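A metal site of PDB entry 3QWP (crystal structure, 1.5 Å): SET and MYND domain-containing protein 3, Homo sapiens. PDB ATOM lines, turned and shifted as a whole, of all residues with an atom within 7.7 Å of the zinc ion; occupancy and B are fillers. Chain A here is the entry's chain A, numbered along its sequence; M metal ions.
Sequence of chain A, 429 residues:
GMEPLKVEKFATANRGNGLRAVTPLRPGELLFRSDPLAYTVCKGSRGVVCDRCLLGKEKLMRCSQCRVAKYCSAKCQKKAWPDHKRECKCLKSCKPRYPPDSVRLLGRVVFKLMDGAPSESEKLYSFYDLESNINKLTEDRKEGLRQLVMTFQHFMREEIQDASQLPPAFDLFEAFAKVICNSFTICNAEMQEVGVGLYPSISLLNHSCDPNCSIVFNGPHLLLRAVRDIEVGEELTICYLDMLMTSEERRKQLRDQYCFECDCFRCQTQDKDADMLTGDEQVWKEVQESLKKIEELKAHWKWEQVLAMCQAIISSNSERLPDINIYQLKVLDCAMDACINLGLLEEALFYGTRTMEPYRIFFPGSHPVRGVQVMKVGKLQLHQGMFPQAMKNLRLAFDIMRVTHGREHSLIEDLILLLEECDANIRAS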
ATOM      1  N   ARG A  62      28.189  21.891  33.617  1.00  0.00           N
ATOM      2  CA  ARG A  62      27.561  22.580  32.509  1.00  0.00           C
ATOM      3  C   ARG A  62      28.487  22.747  31.303  1.00  0.00           C
ATOM      4  O   ARG A  62      29.727  22.782  31.421  1.00  0.00           O
ATOM      5  CB  ARG A  62      26.959  23.906  32.949  1.00  0.00           C
ATOM      6  CG  ARG A  62      27.951  25.017  33.042  1.00  0.00           C
ATOM      7  CD  ARG A  62      27.450  26.064  33.984  1.00  0.00           C
ATOM      8  NE  ARG A  62      28.539  26.923  34.418  1.00  0.00           N
ATOM      9  CZ  ARG A  62      28.352  28.114  34.972  1.00  0.00           C
ATOM     10  NH1 ARG A  62      27.131  28.600  35.102  1.00  0.00           N
ATOM     11  NH2 ARG A  62      29.382  28.821  35.409  1.00  0.00           N
ATOM     12  N   CYS A  63      27.886  22.766  30.122  1.00  0.00           N
ATOM     13  CA  CYS A  63      28.596  23.109  28.900  1.00  0.00           C
ATOM     14  C   CYS A  63      29.058  24.545  29.019  1.00  0.00           C
ATOM     15  O   CYS A  63      28.288  25.462  29.278  1.00  0.00           O
ATOM     16  CB  CYS A  63      27.662  23.006  27.668  1.00  0.00           C
ATOM     17  SG  CYS A  63      28.428  23.557  26.089  1.00  0.00           S
ATOM     18  N   SER A  64      30.337  24.776  28.777  1.00  0.00           N
ATOM     19  CA  SER A  64      30.825  26.115  29.012  1.00  0.00           C
ATOM     20  C   SER A  64      30.319  27.124  27.975  1.00  0.00           C
ATOM     21  O   SER A  64      30.195  28.302  28.281  1.00  0.00           O
ATOM     22  CB  SER A  64      32.333  26.115  29.040  1.00  0.00           C
ATOM     23  OG  SER A  64      32.736  27.426  29.311  1.00  0.00           O
ATOM     24  N   GLN A  65      30.065  26.664  26.756  1.00  0.00           N
ATOM     25  CA  GLN A  65      29.673  27.541  25.639  1.00  0.00           C
ATOM     26  C   GLN A  65      28.246  28.050  25.843  1.00  0.00           C
ATOM     27  O   GLN A  65      27.991  29.260  25.839  1.00  0.00           O
ATOM     28  CB  GLN A  65      29.791  26.825  24.286  1.00  0.00           C
ATOM     29  CG  GLN A  65      31.207  26.712  23.773  1.00  0.00           C
ATOM     30  N   CYS A  66      27.318  27.145  26.125  1.00  0.00           N
ATOM     31  CA  CYS A  66      25.915  27.585  26.268  1.00  0.00           C
ATOM     32  C   CYS A  66      25.450  27.723  27.720  1.00  0.00           C
ATOM     33  O   CYS A  66      24.476  28.443  27.997  1.00  0.00           O
ATOM     34  CB  CYS A  66      24.966  26.647  25.485  1.00  0.00           C
ATOM     35  SG  CYS A  66      24.871  24.950  26.114  1.00  0.00           S
ATOM     36  N   ARG A  67      26.017  26.916  28.611  1.00  0.00           N
ATOM     37  CA  ARG A  67      25.604  26.852  30.000  1.00  0.00           C
ATOM     38  C   ARG A  67      24.182  26.356  30.197  1.00  0.00           C
ATOM     39  O   ARG A  67      23.576  26.564  31.268  1.00  0.00           O
ATOM     40  CB  ARG A  67      25.851  28.203  30.700  1.00  0.00           C
ATOM     41  CG  ARG A  67      27.371  28.421  30.912  1.00  0.00           C
ATOM     42  CD  ARG A  67      27.613  29.741  31.643  1.00  0.00           C
ATOM     43  NE  ARG A  67      29.027  29.882  31.980  1.00  0.00           N
ATOM     44  CZ  ARG A  67      29.497  30.900  32.698  1.00  0.00           C
ATOM     45  NH1 ARG A  67      28.646  31.788  33.199  1.00  0.00           N
ATOM     46  NH2 ARG A  67      30.815  30.957  32.996  1.00  0.00           N
ATOM     47  N   VAL A  68      23.678  25.648  29.187  1.00  0.00           N
ATOM     48  CA  VAL A  68      22.320  25.122  29.248  1.00  0.00           C
ATOM     49  C   VAL A  68      22.379  23.609  29.374  1.00  0.00           C
ATOM     50  O   VAL A  68      21.712  23.020  30.232  1.00  0.00           O
ATOM     51  CB  VAL A  68      21.468  25.562  28.013  1.00  0.00           C
ATOM     52  CG1 VAL A  68      20.134  24.797  27.950  1.00  0.00           C
ATOM     53  CG2 VAL A  68      21.195  27.041  28.088  1.00  0.00           C
ATOM     54  N   ALA A  69      23.157  22.963  28.495  1.00  0.00           N
ATOM     55  CA  ALA A  69      23.370  21.520  28.572  1.00  0.00           C
ATOM     56  C   ALA A  69      24.159  21.207  29.818  1.00  0.00           C
ATOM     57  O   ALA A  69      25.165  21.888  30.080  1.00  0.00           O
ATOM     58  CB  ALA A  69      24.114  21.036  27.316  1.00  0.00           C
ATOM     59  N   LYS A  70      23.732  20.199  30.590  1.00  0.00           N
ATOM     60  CA  LYS A  70      24.458  19.778  31.783  1.00  0.00           C
ATOM     61  C   LYS A  70      24.630  18.275  31.851  1.00  0.00           C
ATOM     62  O   LYS A  70      23.821  17.517  31.295  1.00  0.00           O
ATOM     63  CB  LYS A  70      23.787  20.331  33.054  1.00  0.00           C
ATOM     64  CG  LYS A  70      23.801  21.855  33.114  1.00  0.00           C
ATOM     65  CD  LYS A  70      23.155  22.395  34.368  1.00  0.00           C
ATOM     66  CE  LYS A  70      23.150  23.915  34.396  1.00  0.00           C
ATOM     67  NZ  LYS A  70      22.090  24.447  35.283  1.00  0.00           N
ATOM     68  N   TYR A  71      25.728  17.827  32.439  1.00  0.00           N
ATOM     69  CA  TYR A  71      26.128  16.438  32.300  1.00  0.00           C
ATOM     70  C   TYR A  71      26.630  15.865  33.604  1.00  0.00           C
ATOM     71  O   TYR A  71      27.132  16.610  34.479  1.00  0.00           O
ATOM     72  CB  TYR A  71      27.236  16.320  31.251  1.00  0.00           C
ATOM     73  CG  TYR A  71      26.841  16.894  29.910  1.00  0.00           C
ATOM     74  CD1 TYR A  71      26.070  16.136  29.013  1.00  0.00           C
ATOM     75  CD2 TYR A  71      27.231  18.186  29.522  1.00  0.00           C
ATOM     76  CE1 TYR A  71      25.734  16.626  27.735  1.00  0.00           C
ATOM     77  CE2 TYR A  71      26.868  18.693  28.252  1.00  0.00           C
ATOM     78  CZ  TYR A  71      26.120  17.886  27.379  1.00  0.00           C
ATOM     79  OH  TYR A  71      25.751  18.335  26.113  1.00  0.00           O
ATOM     80  N   GLN A  77      29.490  14.487  28.705  1.00  0.00           N
ATOM     81  CA  GLN A  77      29.564  15.795  28.038  1.00  0.00           C
ATOM     82  C   GLN A  77      30.285  15.612  26.675  1.00  0.00           C
ATOM     83  O   GLN A  77      29.880  16.141  25.626  1.00  0.00           O
ATOM     84  CB  GLN A  77      30.322  16.786  28.894  1.00  0.00           C
ATOM     85  CG  GLN A  77      30.462  18.112  28.202  1.00  0.00           C
ATOM     86  CD  GLN A  77      30.991  19.212  29.069  1.00  0.00           C
ATOM     87  OE1 GLN A  77      31.068  19.070  30.313  1.00  0.00           O
ATOM     88  NE2 GLN A  77      31.294  20.355  28.455  1.00  0.00           N
ATOM     89  N   TRP A  81      28.733  15.731  22.525  1.00  0.00           N
ATOM     90  CA  TRP A  81      29.105  16.946  21.809  1.00  0.00           C
ATOM     91  C   TRP A  81      28.659  16.907  20.346  1.00  0.00           C
ATOM     92  O   TRP A  81      28.123  17.892  19.862  1.00  0.00           O
ATOM     93  CB  TRP A  81      30.617  17.219  21.934  1.00  0.00           C
ATOM     94  CG  TRP A  81      31.045  18.409  21.122  1.00  0.00           C
ATOM     95  CD1 TRP A  81      31.858  18.396  20.020  1.00  0.00           C
ATOM     96  CD2 TRP A  81      30.635  19.772  21.298  1.00  0.00           C
ATOM     97  NE1 TRP A  81      32.028  19.670  19.542  1.00  0.00           N
ATOM     98  CE2 TRP A  81      31.313  20.541  20.324  1.00  0.00           C
ATOM     99  CE3 TRP A  81      29.852  20.432  22.247  1.00  0.00           C
ATOM    100  CZ2 TRP A  81      31.142  21.922  20.196  1.00  0.00           C
ATOM    101  CZ3 TRP A  81      29.686  21.802  22.136  1.00  0.00           C
ATOM    102  CH2 TRP A  81      30.344  22.538  21.125  1.00  0.00           C
ATOM    103  N   HIS A  84      25.112  17.805  20.249  1.00  0.00           N
ATOM    104  CA  HIS A  84      24.845  19.067  20.896  1.00  0.00           C
ATOM    105  C   HIS A  84      25.450  20.313  20.164  1.00  0.00           C
ATOM    106  O   HIS A  84      25.064  21.425  20.427  1.00  0.00           O
ATOM    107  CB  HIS A  84      25.365  19.015  22.340  1.00  0.00           C
ATOM    108  CG  HIS A  84      25.298  20.318  23.086  1.00  0.00           C
ATOM    109  ND1 HIS A  84      24.109  20.934  23.390  1.00  0.00           N
ATOM    110  CD2 HIS A  84      26.267  21.107  23.605  1.00  0.00           C
ATOM    111  CE1 HIS A  84      24.345  22.087  23.978  1.00  0.00           C
ATOM    112  NE2 HIS A  84      25.648  22.192  24.188  1.00  0.00           N
ATOM    113  N   LYS A  85      26.458  20.114  19.321  1.00  0.00           N
ATOM    114  CA  LYS A  85      27.265  21.242  18.885  1.00  0.00           C
ATOM    115  C   LYS A  85      26.511  22.286  18.101  1.00  0.00           C
ATOM    116  O   LYS A  85      26.779  23.473  18.287  1.00  0.00           O
ATOM    117  CB  LYS A  85      28.529  20.786  18.153  1.00  0.00           C
ATOM    118  CG  LYS A  85      28.310  19.937  16.973  1.00  0.00           C
ATOM    119  CD  LYS A  85      29.661  19.482  16.380  1.00  0.00           C
ATOM    120  CE  LYS A  85      30.513  20.678  15.968  1.00  0.00           C
ATOM    121  NZ  LYS A  85      29.791  21.635  15.061  1.00  0.00           N
ATOM    122  N   GLU A  87      23.035  22.829  18.292  1.00  0.00           N
ATOM    123  CA  GLU A  87      22.083  23.468  19.167  1.00  0.00           C
ATOM    124  C   GLU A  87      22.764  24.374  20.169  1.00  0.00           C
ATOM    125  O   GLU A  87      22.140  25.296  20.695  1.00  0.00           O
ATOM    126  CB  GLU A  87      21.153  22.461  19.850  1.00  0.00           C
ATOM    127  CG  GLU A  87      21.825  21.617  20.852  1.00  0.00           C
ATOM    128  CD  GLU A  87      20.894  20.919  21.872  1.00  0.00           C
ATOM    129  OE1 GLU A  87      19.640  20.887  21.736  1.00  0.00           O
ATOM    130  OE2 GLU A  87      21.448  20.332  22.811  1.00  0.00           O
ATOM    131  N   CYS A  88      24.046  24.109  20.449  1.00  0.00           N
ATOM    132  CA  CYS A  88      24.764  24.870  21.450  1.00  0.00           C
ATOM    133  C   CYS A  88      24.799  26.369  21.054  1.00  0.00           C
ATOM    134  O   CYS A  88      24.443  27.220  21.855  1.00  0.00           O
ATOM    135  CB  CYS A  88      26.181  24.273  21.622  1.00  0.00           C
ATOM    136  SG  CYS A  88      27.148  25.139  22.864  1.00  0.00           S
ATOM    137  N   LYS A  89      25.111  26.622  19.786  1.00  0.00           N
ATOM    138  CA  LYS A  89      25.168  27.970  19.221  1.00  0.00           C
ATOM    139  C   LYS A  89      23.791  28.639  19.223  1.00  0.00           C
ATOM    140  O   LYS A  89      23.671  29.836  19.478  1.00  0.00           O
ATOM    141  CB  LYS A  89      25.762  27.969  17.815  1.00  0.00           C
ATOM    142  N   LEU A  91      21.182  27.773  21.422  1.00  0.00           N
ATOM    143  CA  LEU A  91      20.896  27.983  22.829  1.00  0.00           C
ATOM    144  C   LEU A  91      21.698  29.171  23.384  1.00  0.00           C
ATOM    145  O   LEU A  91      21.171  29.950  24.168  1.00  0.00           O
ATOM    146  CB  LEU A  91      21.174  26.710  23.646  1.00  0.00           C
ATOM    147  CG  LEU A  91      20.260  25.475  23.392  1.00  0.00           C
ATOM    148  CD1 LEU A  91      20.964  24.212  23.885  1.00  0.00           C
ATOM    149  CD2 LEU A  91      18.851  25.656  24.052  1.00  0.00           C
ATOM    150  N   LYS A  92      22.956  29.290  22.977  1.00  0.00           N
ATOM    151  CA  LYS A  92      23.797  30.437  23.363  1.00  0.00           C
ATOM    152  C   LYS A  92      23.187  31.734  22.820  1.00  0.00           C
ATOM    153  O   LYS A  92      23.070  32.714  23.553  1.00  0.00           O
ATOM    154  CB  LYS A  92      25.234  30.263  22.867  1.00  0.00           C
ATOM    155  CG  LYS A  92      26.151  31.472  23.153  1.00  0.00           C
ATOM    156  CD  LYS A  92      27.622  31.064  23.222  1.00  0.00           C
ATOM    157  N   ARG A 104      13.215  22.255  20.998  1.00  0.00           N
ATOM    158  CA  ARG A 104      14.557  21.719  21.171  1.00  0.00           C
ATOM    159  C   ARG A 104      14.653  20.300  20.529  1.00  0.00           C
ATOM    160  O   ARG A 104      15.624  19.969  19.815  1.00  0.00           O
ATOM    161  CB  ARG A 104      14.906  21.700  22.658  1.00  0.00           C
ATOM    162  CG  ARG A 104      16.354  21.252  22.857  1.00  0.00           C
ATOM    163  CD  ARG A 104      16.850  21.523  24.292  1.00  0.00           C
ATOM    164  NE  ARG A 104      18.293  21.128  24.391  1.00  0.00           N
ATOM    165  CZ  ARG A 104      18.901  20.926  25.548  1.00  0.00           C
ATOM    166  NH1 ARG A 104      18.267  21.176  26.689  1.00  0.00           N
ATOM    167  NH2 ARG A 104      20.193  20.556  25.557  1.00  0.00           N
HETATM  168 ZN    ZN M   1      26.589  23.922  24.817  1.00  0.00          ZN
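The zinc ion is bound by a ring nitrogen (NE2) of His 84, the side-chain sulfur of Cys 63, the side-chain sulfur of Cys 88 and the side-chain sulfur of Cys 66.
A ring nitrogen (ND1) of His 84 lies within hydrogen-bond range of the side-chain carboxylate (OE2) of Glu 87, 2.8 Å away. N of Gln 65 lies close to SG of Cys 63, 3.6 Å away. The backbone NH (N) of Cys 63 lies within hydrogen-bond range of the backbone carbonyl oxygen (O) of Ala 69 (2.9 Å). The backbone NH (N) of Ala 69 sits close to the side-chain sulfur (SG) of Cys 66, at 3.5 Å. SG of Cys 66 lies close to N of Val 68.
Four residues have an atom within 4 Å of the zinc ion: Cys 63, Cys 66, His 84 and Cys 88. The nearest printed residue that does not touch the zinc ion is Gln 65 (4.4 Å).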
